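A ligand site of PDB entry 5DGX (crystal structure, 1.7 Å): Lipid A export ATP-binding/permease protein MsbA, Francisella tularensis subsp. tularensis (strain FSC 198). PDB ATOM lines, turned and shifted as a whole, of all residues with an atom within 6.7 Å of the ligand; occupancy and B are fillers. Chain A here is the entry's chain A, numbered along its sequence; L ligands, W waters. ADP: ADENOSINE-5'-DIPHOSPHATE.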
ATOM      1  N   PHE A  28      25.377  36.282  29.229  1.00  0.00           N
ATOM      2  CA  PHE A  28      26.727  36.675  29.607  1.00  0.00           C
ATOM      3  C   PHE A  28      26.676  38.199  29.525  1.00  0.00           C
ATOM      4  O   PHE A  28      26.642  38.775  28.425  1.00  0.00           O
ATOM      5  CB  PHE A  28      27.789  36.121  28.686  1.00  0.00           C
ATOM      6  CG  PHE A  28      28.074  34.649  28.884  1.00  0.00           C
ATOM      7  CD1 PHE A  28      28.847  34.226  29.950  1.00  0.00           C
ATOM      8  CD2 PHE A  28      27.634  33.710  27.925  1.00  0.00           C
ATOM      9  CE1 PHE A  28      29.143  32.884  30.100  1.00  0.00           C
ATOM     10  CE2 PHE A  28      27.913  32.368  28.067  1.00  0.00           C
ATOM     11  CZ  PHE A  28      28.679  31.962  29.166  1.00  0.00           C
ATOM     12  N   GLY A  29      26.590  38.871  30.673  1.00  0.00           N
ATOM     13  CA  GLY A  29      26.432  40.340  30.673  1.00  0.00           C
ATOM     14  C   GLY A  29      25.145  40.735  29.960  1.00  0.00           C
ATOM     15  O   GLY A  29      24.070  40.267  30.277  1.00  0.00           O
ATOM     16  N   HIS A  31      24.631  40.071  26.810  1.00  0.00           N
ATOM     17  CA  HIS A  31      24.459  39.146  25.675  1.00  0.00           C
ATOM     18  C   HIS A  31      23.603  37.975  26.113  1.00  0.00           C
ATOM     19  O   HIS A  31      24.076  37.097  26.787  1.00  0.00           O
ATOM     20  CB  HIS A  31      25.808  38.665  25.106  1.00  0.00           C
ATOM     21  CG  HIS A  31      25.707  37.800  23.888  1.00  0.00           C
ATOM     22  ND1 HIS A  31      24.732  37.968  22.909  1.00  0.00           N
ATOM     23  CD2 HIS A  31      26.517  36.814  23.427  1.00  0.00           C
ATOM     24  CE1 HIS A  31      24.896  37.061  21.958  1.00  0.00           C
ATOM     25  NE2 HIS A  31      25.992  36.375  22.227  1.00  0.00           N
ATOM     26  N   VAL A  33      22.117  34.677  25.645  1.00  0.00           N
ATOM     27  CA  VAL A  33      22.506  33.526  24.817  1.00  0.00           C
ATOM     28  C   VAL A  33      21.512  32.353  24.815  1.00  0.00           C
ATOM     29  O   VAL A  33      21.618  31.469  23.968  1.00  0.00           O
ATOM     30  CB  VAL A  33      23.917  33.050  25.181  1.00  0.00           C
ATOM     31  CG1 VAL A  33      24.922  34.183  24.891  1.00  0.00           C
ATOM     32  CG2 VAL A  33      24.001  32.598  26.640  1.00  0.00           C
ATOM     33  N   LEU A  34      20.569  32.382  25.747  1.00  0.00           N
ATOM     34  CA  LEU A  34      19.485  31.421  25.825  1.00  0.00           C
ATOM     35  C   LEU A  34      18.238  32.224  26.209  1.00  0.00           C
ATOM     36  O   LEU A  34      18.295  33.037  27.157  1.00  0.00           O
ATOM     37  CB  LEU A  34      19.790  30.322  26.837  1.00  0.00           C
ATOM     38  CG  LEU A  34      20.897  29.354  26.450  1.00  0.00           C
ATOM     39  CD1 LEU A  34      21.210  28.470  27.650  1.00  0.00           C
ATOM     40  CD2 LEU A  34      20.535  28.461  25.276  1.00  0.00           C
ATOM     41  N   GLY A  51      22.371  23.598  15.644  1.00  0.00           N
ATOM     42  CA  GLY A  51      22.290  25.048  15.430  1.00  0.00           C
ATOM     43  C   GLY A  51      23.650  25.576  15.057  1.00  0.00           C
ATOM     44  O   GLY A  51      24.656  24.917  15.258  1.00  0.00           O
ATOM     45  N   LYS A  52      23.669  26.744  14.440  1.00  0.00           N
ATOM     46  CA  LYS A  52      24.929  27.356  14.096  1.00  0.00           C
ATOM     47  C   LYS A  52      25.766  27.610  15.344  1.00  0.00           C
ATOM     48  O   LYS A  52      25.237  27.764  16.442  1.00  0.00           O
ATOM     49  CB  LYS A  52      24.665  28.687  13.396  1.00  0.00           C
ATOM     50  CG  LYS A  52      23.816  28.545  12.154  1.00  0.00           C
ATOM     51  CD  LYS A  52      23.524  29.898  11.531  1.00  0.00           C
ATOM     52  CE  LYS A  52      22.485  29.791  10.415  1.00  0.00           C
ATOM     53  NZ  LYS A  52      22.912  28.852   9.344  1.00  0.00           N
ATOM     54  N   SER A  53      27.081  27.601  15.179  1.00  0.00           N
ATOM     55  CA  SER A  53      27.984  27.956  16.266  1.00  0.00           C
ATOM     56  C   SER A  53      27.442  29.214  16.917  1.00  0.00           C
ATOM     57  O   SER A  53      26.946  30.125  16.211  1.00  0.00           O
ATOM     58  CB  SER A  53      29.396  28.261  15.743  1.00  0.00           C
ATOM     59  OG  SER A  53      30.237  28.665  16.817  1.00  0.00           O
ATOM     60  N   GLY A  54      27.500  29.285  18.242  1.00  0.00           N
ATOM     61  CA  GLY A  54      26.981  30.433  19.005  1.00  0.00           C
ATOM     62  C   GLY A  54      25.495  30.449  19.340  1.00  0.00           C
ATOM     63  O   GLY A  54      25.020  31.390  19.926  1.00  0.00           O
ATOM     64  N   SER A  55      24.771  29.386  18.966  1.00  0.00           N
ATOM     65  CA  SER A  55      23.338  29.289  19.222  1.00  0.00           C
ATOM     66  C   SER A  55      22.979  29.013  20.686  1.00  0.00           C
ATOM     67  O   SER A  55      21.803  29.027  21.051  1.00  0.00           O
ATOM     68  CB  SER A  55      22.736  28.174  18.363  1.00  0.00           C
ATOM     69  OG  SER A  55      22.821  28.459  16.972  1.00  0.00           O
ATOM     70  N   GLY A  56      23.985  28.719  21.523  1.00  0.00           N
ATOM     71  CA  GLY A  56      23.772  28.463  22.960  1.00  0.00           C
ATOM     72  C   GLY A  56      23.787  27.023  23.405  1.00  0.00           C
ATOM     73  O   GLY A  56      23.501  26.705  24.580  1.00  0.00           O
ATOM     74  N   LYS A  57      24.180  26.126  22.509  1.00  0.00           N
ATOM     75  CA  LYS A  57      24.119  24.678  22.759  1.00  0.00           C
ATOM     76  C   LYS A  57      25.033  24.219  23.919  1.00  0.00           C
ATOM     77  O   LYS A  57      24.595  23.500  24.811  1.00  0.00           O
ATOM     78  CB  LYS A  57      24.456  23.891  21.471  1.00  0.00           C
ATOM     79  CG  LYS A  57      23.575  24.276  20.290  1.00  0.00           C
ATOM     80  CD  LYS A  57      23.749  23.480  18.999  1.00  0.00           C
ATOM     81  CE  LYS A  57      25.164  23.423  18.452  1.00  0.00           C
ATOM     82  NZ  LYS A  57      25.725  24.746  18.128  1.00  0.00           N
ATOM     83  N   THR A  58      26.300  24.625  23.877  1.00  0.00           N
ATOM     84  CA  THR A  58      27.271  24.263  24.899  1.00  0.00           C
ATOM     85  C   THR A  58      26.839  24.848  26.252  1.00  0.00           C
ATOM     86  O   THR A  58      26.869  24.173  27.299  1.00  0.00           O
ATOM     87  CB  THR A  58      28.672  24.761  24.507  1.00  0.00           C
ATOM     88  OG1 THR A  58      29.035  24.180  23.237  1.00  0.00           O
ATOM     89  CG2 THR A  58      29.736  24.394  25.547  1.00  0.00           C
ATOM     90  N   THR A  59      26.413  26.106  26.219  1.00  0.00           N
ATOM     91  CA  THR A  59      26.021  26.802  27.429  1.00  0.00           C
ATOM     92  C   THR A  59      24.818  26.113  28.052  1.00  0.00           C
ATOM     93  O   THR A  59      24.819  25.891  29.266  1.00  0.00           O
ATOM     94  CB  THR A  59      25.723  28.279  27.107  1.00  0.00           C
ATOM     95  OG1 THR A  59      26.948  28.884  26.701  1.00  0.00           O
ATOM     96  CG2 THR A  59      25.174  29.026  28.301  1.00  0.00           C
ATOM     97  N   LEU A  60      23.862  25.686  27.218  1.00  0.00           N
ATOM     98  CA  LEU A  60      22.695  24.945  27.730  1.00  0.00           C
ATOM     99  C   LEU A  60      23.148  23.672  28.491  1.00  0.00           C
ATOM    100  O   LEU A  60      22.680  23.403  29.606  1.00  0.00           O
ATOM    101  CB  LEU A  60      21.724  24.598  26.609  1.00  0.00           C
ATOM    102  CG  LEU A  60      20.460  23.778  26.954  1.00  0.00           C
ATOM    103  CD1 LEU A  60      19.633  24.433  28.045  1.00  0.00           C
ATOM    104  CD2 LEU A  60      19.626  23.544  25.715  1.00  0.00           C
ATOM    105  N   TYR A  68      27.120  26.633  35.137  1.00  0.00           N
ATOM    106  CA  TYR A  68      26.557  28.010  35.077  1.00  0.00           C
ATOM    107  C   TYR A  68      25.144  27.888  35.625  1.00  0.00           C
ATOM    108  O   TYR A  68      24.558  26.782  35.619  1.00  0.00           O
ATOM    109  CB  TYR A  68      26.444  28.575  33.659  1.00  0.00           C
ATOM    110  CG  TYR A  68      27.742  28.922  33.010  1.00  0.00           C
ATOM    111  CD1 TYR A  68      28.463  29.993  33.461  1.00  0.00           C
ATOM    112  CD2 TYR A  68      28.222  28.227  31.913  1.00  0.00           C
ATOM    113  CE1 TYR A  68      29.670  30.349  32.901  1.00  0.00           C
ATOM    114  CE2 TYR A  68      29.440  28.573  31.329  1.00  0.00           C
ATOM    115  CZ  TYR A  68      30.152  29.641  31.843  1.00  0.00           C
ATOM    116  OH  TYR A  68      31.347  30.066  31.299  1.00  0.00           O
ATOM    117  N   ILE A 210      24.861  17.206  21.438  1.00  0.00           N
ATOM    118  CA  ILE A 210      25.124  18.356  20.615  1.00  0.00           C
ATOM    119  C   ILE A 210      25.662  17.682  19.362  1.00  0.00           C
ATOM    120  O   ILE A 210      26.845  17.199  19.331  1.00  0.00           O
ATOM    121  CB  ILE A 210      26.164  19.274  21.237  1.00  0.00           C
ATOM    122  CG1 ILE A 210      25.701  19.736  22.626  1.00  0.00           C
ATOM    123  CG2 ILE A 210      26.450  20.423  20.293  1.00  0.00           C
ATOM    124  CD1 ILE A 210      26.697  20.693  23.262  1.00  0.00           C
ATOM    125  N   MET A 226      18.182  25.040  17.487  1.00  0.00           N
ATOM    126  CA  MET A 226      18.419  26.328  18.164  1.00  0.00           C
ATOM    127  C   MET A 226      18.931  27.422  17.193  1.00  0.00           C
ATOM    128  O   MET A 226      19.645  27.164  16.228  1.00  0.00           O
ATOM    129  CB  MET A 226      19.353  26.123  19.362  1.00  0.00           C
ATOM    130  CG  MET A 226      18.715  25.292  20.483  1.00  0.00           C
ATOM    131  SD  MET A 226      19.845  24.867  21.824  1.00  0.00           S
ATOM    132  CE  MET A 226      19.999  26.439  22.670  1.00  0.00           C
HETATM  133  PB  ADP L   1      27.261  26.825  20.624  1.00  0.00           P
HETATM  134  O1B ADP L   1      27.720  25.687  21.530  1.00  0.00           O
HETATM  135  O2B ADP L   1      25.880  26.743  20.130  1.00  0.00           O
HETATM  136  O3B ADP L   1      28.367  27.189  19.669  1.00  0.00           O
HETATM  137  PA  ADP L   1      27.836  28.494  22.987  1.00  0.00           P
HETATM  138  O1A ADP L   1      29.248  27.991  23.024  1.00  0.00           O
HETATM  139  O2A ADP L   1      26.869  28.243  24.089  1.00  0.00           O
HETATM  140  O3A ADP L   1      27.105  28.135  21.572  1.00  0.00           O
HETATM  141  O5' ADP L   1      27.962  30.112  22.911  1.00  0.00           O
HETATM  142  C5' ADP L   1      26.821  30.922  23.017  1.00  0.00           C
HETATM  143  C4' ADP L   1      27.246  32.397  23.000  1.00  0.00           C
HETATM  144  O4' ADP L   1      27.808  32.674  24.282  1.00  0.00           O
HETATM  145  C3' ADP L   1      28.320  32.729  21.961  1.00  0.00           C
HETATM  146  O3' ADP L   1      28.018  33.985  21.357  1.00  0.00           O
HETATM  147  C2' ADP L   1      29.604  32.837  22.757  1.00  0.00           C
HETATM  148  O2' ADP L   1      30.559  33.769  22.230  1.00  0.00           O
HETATM  149  C1' ADP L   1      29.078  33.303  24.100  1.00  0.00           C
HETATM  150  N9  ADP L   1      29.973  32.931  25.209  1.00  0.00           N
HETATM  151  C8  ADP L   1      30.391  31.685  25.513  1.00  0.00           C
HETATM  152  N7  ADP L   1      31.176  31.703  26.612  1.00  0.00           N
HETATM  153  C5  ADP L   1      31.248  32.996  27.024  1.00  0.00           C
HETATM  154  C6  ADP L   1      31.902  33.718  28.117  1.00  0.00           C
HETATM  155  N6  ADP L   1      32.649  33.014  29.006  1.00  0.00           N
HETATM  156  N1  ADP L   1      31.721  35.063  28.206  1.00  0.00           N
HETATM  157  C2  ADP L   1      30.984  35.741  27.308  1.00  0.00           C
HETATM  158  N3  ADP L   1      30.350  35.135  26.259  1.00  0.00           N
HETATM  159  C4  ADP L   1      30.452  33.790  26.093  1.00  0.00           C
HETATM  160  O   HOH W   1      32.875  31.786  23.129  1.00  0.00           O
HETATM  161  O   HOH W   2      31.049  25.720  22.097  1.00  0.00           O
HETATM  162  O   HOH W   3      32.754  32.048  32.301  1.00  0.00           O
HETATM  163  O   HOH W   4      30.721  25.882  18.916  1.00  0.00           O
HETATM  164  O   HOH W   5      29.170  37.212  24.709  1.00  0.00           O
HETATM  165  O   HOH W   6      30.934  27.989  25.090  1.00  0.00           O
HETATM  166  O   HOH W   7      30.426  28.943  20.211  1.00  0.00           O
HETATM  167  O   HOH W   8      32.874  37.041  29.775  1.00  0.00           O
HETATM  168  O   HOH W   9      31.522  29.580  28.522  1.00  0.00           O
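An oxygen (O2B) of the ligand lies within hydrogen-bond range of the backbone NH (N) of Lys 57, at 3.0 Å.
O2B of the ligand lies within hydrogen-bond range of N of Gly 56 (3.1 Å).
The side-chain hydroxyl (OG1) of Thr 58 lies within hydrogen-bond range of an oxygen (O1B) of the ligand (2.6 Å).
The backbone NH (N) of Thr 58 lies within hydrogen-bond range of an oxygen (O1B) of the ligand, at 2.9 Å.
O2A of the ligand lies within hydrogen-bond range of N of Thr 59 (3.1 Å).
An oxygen (O3') of the ligand sits at hydrogen-bond distance from a ring nitrogen (NE2) of His 31 (3.3 Å).
The backbone NH of Ser 55 lies within hydrogen-bond range of an oxygen (O2B) of the ligand, 3.1 Å away.
The side-chain amino group (NZ) of Lys 57 lies within salt-bridge range of an oxygen (O2B) of the ligand, at 2.8 Å.
O2A of the ligand lies within hydrogen-bond range of OG1 of Thr 59 (2.7 Å).
O3B of the ligand lies within hydrogen-bond range of N of Gly 54 (2.7 Å).
Residues that only touch the ligand: Phe 28, Val 33, Lys 52, Ser 53 and Tyr 68.
Hydrophobic or aromatic side chains within 4 Å of the ligand: Phe 28, His 31 and Val 33.
The backbone carbonyl oxygen of Lys 52 lies within hydrogen-bond range of the side-chain hydroxyl of Ser 55, at 2.6 Å.
The backbone carbonyl oxygen (O) of Gly 51 sits at hydrogen-bond distance from the side-chain amino group (NZ) of Lys 57 (3.1 Å).
O of Lys 52 is in hydrogen-bond range of NZ of Lys 57 (3.5 Å).
Water W7 lies within hydrogen-bond range of an oxygen (O3B) of the ligand (2.8 Å) and the side-chain hydroxyl of Ser 53 (3.4 Å).
Water W9 lies within hydrogen-bond range of the side-chain hydroxyl (OH) of Tyr 68 (2.8 Å) and a nitrogen (N7) of the ligand (2.9 Å).
Water W2 bridges the side-chain hydroxyl (OG1) of Thr 58 and an oxygen (O1A) of the ligand.
Water W3 lies within hydrogen-bond range of OH of Tyr 68 (2.6 Å) and N6 of the ligand (3.4 Å).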
